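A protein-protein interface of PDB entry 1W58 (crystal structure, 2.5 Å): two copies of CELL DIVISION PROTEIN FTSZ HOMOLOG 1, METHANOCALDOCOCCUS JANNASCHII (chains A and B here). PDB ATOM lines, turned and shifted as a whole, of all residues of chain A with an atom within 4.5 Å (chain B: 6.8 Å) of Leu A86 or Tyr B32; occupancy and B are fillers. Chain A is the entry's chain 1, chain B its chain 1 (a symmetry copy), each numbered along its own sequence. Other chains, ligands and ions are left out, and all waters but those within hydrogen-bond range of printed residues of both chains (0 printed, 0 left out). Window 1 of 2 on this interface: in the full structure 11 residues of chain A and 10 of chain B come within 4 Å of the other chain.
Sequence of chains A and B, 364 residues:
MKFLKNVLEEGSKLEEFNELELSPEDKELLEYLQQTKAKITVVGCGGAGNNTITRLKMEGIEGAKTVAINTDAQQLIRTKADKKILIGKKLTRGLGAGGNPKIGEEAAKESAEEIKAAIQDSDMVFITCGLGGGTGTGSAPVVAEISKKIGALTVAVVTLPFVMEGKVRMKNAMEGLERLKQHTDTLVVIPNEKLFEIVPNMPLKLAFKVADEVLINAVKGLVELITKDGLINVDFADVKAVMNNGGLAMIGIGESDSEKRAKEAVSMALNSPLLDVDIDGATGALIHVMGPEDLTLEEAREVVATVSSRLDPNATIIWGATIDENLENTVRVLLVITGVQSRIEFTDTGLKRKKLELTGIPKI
The side-chain hydroxyl (OH) of Tyr B32 is in hydrogen-bond range of the backbone carbonyl oxygen (O) of Lys A89 (2.6 Å).
The backbone NH (N) of Ala A73 is in hydrogen-bond range of the backbone carbonyl oxygen (O) of Gly A94 (2.8 Å).
Among the printed residues, pairs that only touch across the chains: Ala A73 with Leu B33, Leu A86 with Tyr B32 and Arg A93 with Tyr B32.
Printed residues of chain B within 4 Å of Ala A73: Leu B33 (3.9 Å).
Of the printed residues of chain B, Lys A89 touches Tyr B32 (2.6 Å).
Printed residues of chain B within 4 Å of Arg A93: Tyr B32.
Leu B30 touches none of the printed residues of chain A.
Tyr B32 touches just these residues of chain A: Leu A86 (3.8 Å), Lys A89 (2.6 Å) and Arg A93 (3.7 Å).
Of the printed residues of chain A, Leu B33 touches Ala A73.
The nearest residue of chain B that does not touch Leu A86 is Leu B29 (4.2 Å).
The nearest residue of chain A that does not touch Tyr B32 is Gly A94 (4.2 Å).
The nearest printed residue of chain B that does not touch Ala A73 is Leu B29 (5.1 Å).
Of the 12 printed residues of chain B, 2 touch a printed residue of chain A.
Hydrophobic or aromatic side chains of chain B that line the printed part of chain A: Tyr B32 and Leu B33.
Of the 14 printed residues of chain A, 4 touch a printed residue of chain B.
Hydrophobic or aromatic side chains of chain A within 4 Å of the printed part of chain B: Ala A73 and Leu A86.
Among the printed residues, 4 pairs touch across the chains.
Among the printed residues, no Asp or Glu carboxylate lies within 4 Å of a Lys or Arg side-chain nitrogen of the other chain.
No position is printed for both chains.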
ATOM      1  N   ASN A  70      15.468  16.291  16.477  1.00  0.00           N
ATOM      2  CA  ASN A  70      14.759  15.036  16.490  1.00  0.00           C
ATOM      3  C   ASN A  70      13.919  14.871  17.731  1.00  0.00           C
ATOM      4  O   ASN A  70      14.114  15.511  18.772  1.00  0.00           O
ATOM      5  CB  ASN A  70      15.754  13.876  16.377  1.00  0.00           C
ATOM      6  CG  ASN A  70      15.226  12.725  15.539  1.00  0.00           C
ATOM      7  OD1 ASN A  70      15.969  12.113  14.775  1.00  0.00           O
ATOM      8  ND2 ASN A  70      13.948  12.424  15.679  1.00  0.00           N
ATOM      9  N   THR A  71      12.972  13.973  17.581  1.00  0.00           N
ATOM     10  CA  THR A  71      12.037  13.614  18.613  1.00  0.00           C
ATOM     11  C   THR A  71      12.634  12.352  19.284  1.00  0.00           C
ATOM     12  O   THR A  71      12.334  12.057  20.442  1.00  0.00           O
ATOM     13  CB  THR A  71      10.740  13.338  17.906  1.00  0.00           C
ATOM     14  OG1 THR A  71       9.632  13.767  18.689  1.00  0.00           O
ATOM     15  CG2 THR A  71      10.665  11.945  17.551  1.00  0.00           C
ATOM     16  N   ASP A  72      13.505  11.645  18.538  1.00  0.00           N
ATOM     17  CA  ASP A  72      14.207  10.415  18.971  1.00  0.00           C
ATOM     18  C   ASP A  72      15.606  10.703  19.551  1.00  0.00           C
ATOM     19  O   ASP A  72      16.533  11.040  18.819  1.00  0.00           O
ATOM     20  CB  ASP A  72      14.367   9.460  17.778  1.00  0.00           C
ATOM     21  CG  ASP A  72      14.973   8.097  18.166  1.00  0.00           C
ATOM     22  OD1 ASP A  72      16.072   8.032  18.748  1.00  0.00           O
ATOM     23  OD2 ASP A  72      14.344   7.071  17.871  1.00  0.00           O
ATOM     24  N   ALA A  73      15.772  10.530  20.855  1.00  0.00           N
ATOM     25  CA  ALA A  73      17.054  10.801  21.483  1.00  0.00           C
ATOM     26  C   ALA A  73      18.254   9.990  20.950  1.00  0.00           C
ATOM     27  O   ALA A  73      19.342  10.541  20.715  1.00  0.00           O
ATOM     28  CB  ALA A  73      16.922  10.612  22.973  1.00  0.00           C
ATOM     29  N   LEU A  76      19.511  11.269  17.740  1.00  0.00           N
ATOM     30  CA  LEU A  76      20.161  12.556  17.939  1.00  0.00           C
ATOM     31  C   LEU A  76      21.554  12.352  18.538  1.00  0.00           C
ATOM     32  O   LEU A  76      22.493  13.068  18.181  1.00  0.00           O
ATOM     33  CB  LEU A  76      19.301  13.440  18.857  1.00  0.00           C
ATOM     34  CG  LEU A  76      19.491  14.955  18.798  1.00  0.00           C
ATOM     35  CD1 LEU A  76      19.333  15.410  17.342  1.00  0.00           C
ATOM     36  CD2 LEU A  76      18.457  15.650  19.687  1.00  0.00           C
ATOM     37  N   LYS A  84      22.423  20.442  18.477  1.00  0.00           N
ATOM     38  CA  LYS A  84      21.373  19.437  18.533  1.00  0.00           C
ATOM     39  C   LYS A  84      20.218  19.896  19.413  1.00  0.00           C
ATOM     40  O   LYS A  84      20.427  20.487  20.467  1.00  0.00           O
ATOM     41  CB  LYS A  84      21.912  18.132  19.089  1.00  0.00           C
ATOM     42  CG  LYS A  84      23.162  17.612  18.404  1.00  0.00           C
ATOM     43  CD  LYS A  84      23.563  16.270  19.024  1.00  0.00           C
ATOM     44  CE  LYS A  84      24.822  15.712  18.417  1.00  0.00           C
ATOM     45  NZ  LYS A  84      25.090  14.352  18.944  1.00  0.00           N
ATOM     46  N   ILE A  85      18.998  19.614  18.983  1.00  0.00           N
ATOM     47  CA  ILE A  85      17.830  19.988  19.768  1.00  0.00           C
ATOM     48  C   ILE A  85      16.859  18.792  19.833  1.00  0.00           C
ATOM     49  O   ILE A  85      16.436  18.267  18.798  1.00  0.00           O
ATOM     50  CB  ILE A  85      17.063  21.181  19.133  1.00  0.00           C
ATOM     51  CG1 ILE A  85      17.989  22.372  18.900  1.00  0.00           C
ATOM     52  CG2 ILE A  85      15.925  21.601  20.034  1.00  0.00           C
ATOM     53  CD1 ILE A  85      17.248  23.584  18.384  1.00  0.00           C
ATOM     54  N   LEU A  86      16.522  18.357  21.046  1.00  0.00           N
ATOM     55  CA  LEU A  86      15.580  17.271  21.226  1.00  0.00           C
ATOM     56  C   LEU A  86      14.245  17.982  21.329  1.00  0.00           C
ATOM     57  O   LEU A  86      14.010  18.721  22.275  1.00  0.00           O
ATOM     58  CB  LEU A  86      15.867  16.511  22.524  1.00  0.00           C
ATOM     59  CG  LEU A  86      15.024  15.263  22.843  1.00  0.00           C
ATOM     60  CD1 LEU A  86      15.350  14.157  21.825  1.00  0.00           C
ATOM     61  CD2 LEU A  86      15.338  14.783  24.292  1.00  0.00           C
ATOM     62  N   ILE A  87      13.370  17.776  20.361  1.00  0.00           N
ATOM     63  CA  ILE A  87      12.084  18.456  20.398  1.00  0.00           C
ATOM     64  C   ILE A  87      11.004  17.542  20.953  1.00  0.00           C
ATOM     65  O   ILE A  87      11.141  16.326  20.915  1.00  0.00           O
ATOM     66  CB  ILE A  87      11.671  18.969  18.974  1.00  0.00           C
ATOM     67  CG1 ILE A  87      11.515  17.794  18.012  1.00  0.00           C
ATOM     68  CG2 ILE A  87      12.723  19.937  18.449  1.00  0.00           C
ATOM     69  CD1 ILE A  87      10.724  18.115  16.722  1.00  0.00           C
ATOM     70  N   GLY A  88       9.932  18.137  21.465  1.00  0.00           N
ATOM     71  CA  GLY A  88       8.840  17.370  22.032  1.00  0.00           C
ATOM     72  C   GLY A  88       9.179  16.614  23.306  1.00  0.00           C
ATOM     73  O   GLY A  88       8.613  15.554  23.552  1.00  0.00           O
ATOM     74  N   LYS A  89      10.076  17.140  24.131  1.00  0.00           N
ATOM     75  CA  LYS A  89      10.446  16.447  25.364  1.00  0.00           C
ATOM     76  C   LYS A  89       9.303  16.049  26.296  1.00  0.00           C
ATOM     77  O   LYS A  89       9.380  15.031  26.978  1.00  0.00           O
ATOM     78  CB  LYS A  89      11.475  17.255  26.151  1.00  0.00           C
ATOM     79  CG  LYS A  89      12.850  17.119  25.541  1.00  0.00           C
ATOM     80  CD  LYS A  89      13.954  17.509  26.485  1.00  0.00           C
ATOM     81  CE  LYS A  89      13.946  18.987  26.776  1.00  0.00           C
ATOM     82  NZ  LYS A  89      15.180  19.365  27.531  1.00  0.00           N
ATOM     83  N   ARG A  93       8.950  11.197  24.591  1.00  0.00           N
ATOM     84  CA  ARG A  93       9.897  11.464  25.669  1.00  0.00           C
ATOM     85  C   ARG A  93      11.272  11.044  25.253  1.00  0.00           C
ATOM     86  O   ARG A  93      11.924  10.262  25.935  1.00  0.00           O
ATOM     87  CB  ARG A  93       9.463  10.759  26.951  1.00  0.00           C
ATOM     88  CG  ARG A  93       8.234  11.396  27.594  1.00  0.00           C
ATOM     89  CD  ARG A  93       7.798  10.665  28.858  1.00  0.00           C
ATOM     90  NE  ARG A  93       7.271   9.325  28.575  1.00  0.00           N
ATOM     91  CZ  ARG A  93       7.074   8.381  29.496  1.00  0.00           C
ATOM     92  NH1 ARG A  93       7.363   8.621  30.775  1.00  0.00           N
ATOM     93  NH2 ARG A  93       6.586   7.194  29.139  1.00  0.00           N
ATOM     94  N   GLY A  94      11.696  11.593  24.120  1.00  0.00           N
ATOM     95  CA  GLY A  94      12.986  11.272  23.551  1.00  0.00           C
ATOM     96  C   GLY A  94      12.875   9.907  22.906  1.00  0.00           C
ATOM     97  O   GLY A  94      13.868   9.312  22.521  1.00  0.00           O
ATOM     98  N   SER A 111       8.649  23.081  21.144  1.00  0.00           N
ATOM     99  CA  SER A 111      10.021  23.571  21.323  1.00  0.00           C
ATOM    100  C   SER A 111      10.372  24.760  20.395  1.00  0.00           C
ATOM    101  O   SER A 111      11.547  25.001  20.125  1.00  0.00           O
ATOM    102  CB  SER A 111      11.023  22.436  21.072  1.00  0.00           C
ATOM    103  OG  SER A 111      10.679  21.235  21.754  1.00  0.00           O
ATOM    104  N   LYS B  27      26.015  14.243  26.592  1.00  0.00           N
ATOM    105  CA  LYS B  27      25.886  13.830  27.994  1.00  0.00           C
ATOM    106  C   LYS B  27      24.572  14.299  28.551  1.00  0.00           C
ATOM    107  O   LYS B  27      23.965  13.650  29.392  1.00  0.00           O
ATOM    108  CB  LYS B  27      26.997  14.435  28.857  1.00  0.00           C
ATOM    109  CG  LYS B  27      28.397  13.919  28.585  1.00  0.00           C
ATOM    110  CD  LYS B  27      29.397  14.663  29.459  1.00  0.00           C
ATOM    111  CE  LYS B  27      30.837  14.255  29.178  1.00  0.00           C
ATOM    112  NZ  LYS B  27      31.777  15.024  30.043  1.00  0.00           N
ATOM    113  N   GLU B  28      24.160  15.462  28.079  1.00  0.00           N
ATOM    114  CA  GLU B  28      22.921  16.107  28.485  1.00  0.00           C
ATOM    115  C   GLU B  28      21.728  15.281  27.975  1.00  0.00           C
ATOM    116  O   GLU B  28      20.741  15.080  28.690  1.00  0.00           O
ATOM    117  CB  GLU B  28      22.921  17.503  27.870  1.00  0.00           C
ATOM    118  CG  GLU B  28      22.037  18.544  28.494  1.00  0.00           C
ATOM    119  CD  GLU B  28      22.315  19.904  27.873  1.00  0.00           C
ATOM    120  OE1 GLU B  28      23.450  20.406  28.045  1.00  0.00           O
ATOM    121  OE2 GLU B  28      21.416  20.458  27.203  1.00  0.00           O
ATOM    122  N   LEU B  29      21.834  14.818  26.732  1.00  0.00           N
ATOM    123  CA  LEU B  29      20.806  13.996  26.101  1.00  0.00           C
ATOM    124  C   LEU B  29      20.665  12.633  26.814  1.00  0.00           C
ATOM    125  O   LEU B  29      19.545  12.153  27.019  1.00  0.00           O
ATOM    126  CB  LEU B  29      21.157  13.788  24.624  1.00  0.00           C
ATOM    127  CG  LEU B  29      20.465  14.617  23.536  1.00  0.00           C
ATOM    128  CD1 LEU B  29      19.652  15.750  24.136  1.00  0.00           C
ATOM    129  CD2 LEU B  29      21.515  15.128  22.568  1.00  0.00           C
ATOM    130  N   LEU B  30      21.796  12.025  27.188  1.00  0.00           N
ATOM    131  CA  LEU B  30      21.795  10.743  27.904  1.00  0.00           C
ATOM    132  C   LEU B  30      21.114  10.905  29.274  1.00  0.00           C
ATOM    133  O   LEU B  30      20.249  10.121  29.653  1.00  0.00           O
ATOM    134  CB  LEU B  30      23.230  10.219  28.102  1.00  0.00           C
ATOM    135  CG  LEU B  30      23.979   9.324  27.090  1.00  0.00           C
ATOM    136  CD1 LEU B  30      23.013   8.560  26.188  1.00  0.00           C
ATOM    137  CD2 LEU B  30      24.901  10.152  26.260  1.00  0.00           C
ATOM    138  N   GLU B  31      21.505  11.939  30.011  1.00  0.00           N
ATOM    139  CA  GLU B  31      20.930  12.206  31.325  1.00  0.00           C
ATOM    140  C   GLU B  31      19.414  12.338  31.261  1.00  0.00           C
ATOM    141  O   GLU B  31      18.699  11.870  32.138  1.00  0.00           O
ATOM    142  CB  GLU B  31      21.528  13.491  31.908  1.00  0.00           C
ATOM    143  CG  GLU B  31      22.539  13.273  33.035  1.00  0.00           C
ATOM    144  CD  GLU B  31      21.896  12.711  34.311  1.00  0.00           C
ATOM    145  OE1 GLU B  31      22.108  11.511  34.631  1.00  0.00           O
ATOM    146  OE2 GLU B  31      21.171  13.478  34.993  1.00  0.00           O
ATOM    147  N   TYR B  32      18.921  12.987  30.220  1.00  0.00           N
ATOM    148  CA  TYR B  32      17.494  13.161  30.080  1.00  0.00           C
ATOM    149  C   TYR B  32      16.809  11.802  30.044  1.00  0.00           C
ATOM    150  O   TYR B  32      15.740  11.623  30.621  1.00  0.00           O
ATOM    151  CB  TYR B  32      17.162  13.910  28.785  1.00  0.00           C
ATOM    152  CG  TYR B  32      15.681  13.969  28.534  1.00  0.00           C
ATOM    153  CD1 TYR B  32      14.873  14.861  29.237  1.00  0.00           C
ATOM    154  CD2 TYR B  32      15.076  13.098  27.635  1.00  0.00           C
ATOM    155  CE1 TYR B  32      13.502  14.882  29.053  1.00  0.00           C
ATOM    156  CE2 TYR B  32      13.702  13.108  27.444  1.00  0.00           C
ATOM    157  CZ  TYR B  32      12.918  14.003  28.153  1.00  0.00           C
ATOM    158  OH  TYR B  32      11.548  14.011  27.969  1.00  0.00           O
ATOM    159  N   LEU B  33      17.410  10.850  29.338  1.00  0.00           N
ATOM    160  CA  LEU B  33      16.801   9.540  29.242  1.00  0.00           C
ATOM    161  C   LEU B  33      16.726   8.853  30.616  1.00  0.00           C
ATOM    162  O   LEU B  33      15.854   8.006  30.836  1.00  0.00           O
ATOM    163  CB  LEU B  33      17.570   8.671  28.239  1.00  0.00           C
ATOM    164  CG  LEU B  33      17.402   9.061  26.758  1.00  0.00           C
ATOM    165  CD1 LEU B  33      18.303   8.215  25.894  1.00  0.00           C
ATOM    166  CD2 LEU B  33      15.955   8.877  26.339  1.00  0.00           C
ATOM    167  N   GLN B  34      17.619   9.226  31.538  1.00  0.00           N
ATOM    168  CA  GLN B  34      17.633   8.629  32.880  1.00  0.00           C
ATOM    169  C   GLN B  34      16.664   9.291  33.843  1.00  0.00           C
ATOM    170  O   GLN B  34      16.558   8.876  34.994  1.00  0.00           O
ATOM    171  CB  GLN B  34      19.028   8.698  33.507  1.00  0.00           C
ATOM    172  CG  GLN B  34      20.086   7.959  32.753  1.00  0.00           C
ATOM    173  CD  GLN B  34      19.730   6.507  32.572  1.00  0.00           C
ATOM    174  OE1 GLN B  34      19.297   5.842  33.521  1.00  0.00           O
ATOM    175  NE2 GLN B  34      19.912   5.996  31.352  1.00  0.00           N
ATOM    176  N   GLN B  35      15.962  10.322  33.392  1.00  0.00           N
ATOM    177  CA  GLN B  35      15.036  11.008  34.282  1.00  0.00           C
ATOM    178  C   GLN B  35      14.025  10.010  34.790  1.00  0.00           C
ATOM    179  O   GLN B  35      13.480   9.208  34.032  1.00  0.00           O
ATOM    180  CB  GLN B  35      14.332  12.154  33.567  1.00  0.00           C
ATOM    181  CG  GLN B  35      13.532  13.061  34.489  1.00  0.00           C
ATOM    182  CD  GLN B  35      13.059  14.341  33.799  1.00  0.00           C
ATOM    183  OE1 GLN B  35      13.855  15.040  33.146  1.00  0.00           O
ATOM    184  NE2 GLN B  35      11.766  14.659  33.952  1.00  0.00           N
ATOM    185  N   THR B  36      13.764  10.066  36.083  1.00  0.00           N
ATOM    186  CA  THR B  36      12.842   9.126  36.677  1.00  0.00           C
ATOM    187  C   THR B  36      11.482   9.664  37.123  1.00  0.00           C
ATOM    188  O   THR B  36      10.473   8.979  36.995  1.00  0.00           O
ATOM    189  CB  THR B  36      13.515   8.404  37.870  1.00  0.00           C
ATOM    190  OG1 THR B  36      12.563   8.278  38.927  1.00  0.00           O
ATOM    191  CG2 THR B  36      14.756   9.170  38.369  1.00  0.00           C
ATOM    192  N   LYS B  39       8.197  16.156  36.609  1.00  0.00           N
ATOM    193  CA  LYS B  39       8.425  17.425  37.274  1.00  0.00           C
ATOM    194  C   LYS B  39       7.085  18.146  37.370  1.00  0.00           C
ATOM    195  O   LYS B  39       6.446  18.404  36.346  1.00  0.00           O
ATOM    196  CB  LYS B  39       9.456  18.241  36.495  1.00  0.00           C
ATOM    197  CG  LYS B  39      10.877  17.704  36.669  1.00  0.00           C
ATOM    198  CD  LYS B  39      11.930  18.741  36.284  1.00  0.00           C
ATOM    199  CE  LYS B  39      12.504  18.450  34.922  1.00  0.00           C
ATOM    200  NZ  LYS B  39      11.410  18.175  33.963  1.00  0.00           N
ATOM    201  N   ASP B 123       6.518  19.143  33.571  1.00  0.00           N
ATOM    202  CA  ASP B 123       5.843  18.063  32.859  1.00  0.00           C
ATOM    203  C   ASP B 123       4.367  18.202  33.170  1.00  0.00           C
ATOM    204  O   ASP B 123       3.519  17.834  32.369  1.00  0.00           O
ATOM    205  CB  ASP B 123       6.286  16.685  33.369  1.00  0.00           C
ATOM    206  CG  ASP B 123       7.696  16.289  32.922  1.00  0.00           C
ATOM    207  OD1 ASP B 123       8.590  16.193  33.794  1.00  0.00           O
ATOM    208  OD2 ASP B 123       7.901  16.052  31.707  1.00  0.00           O
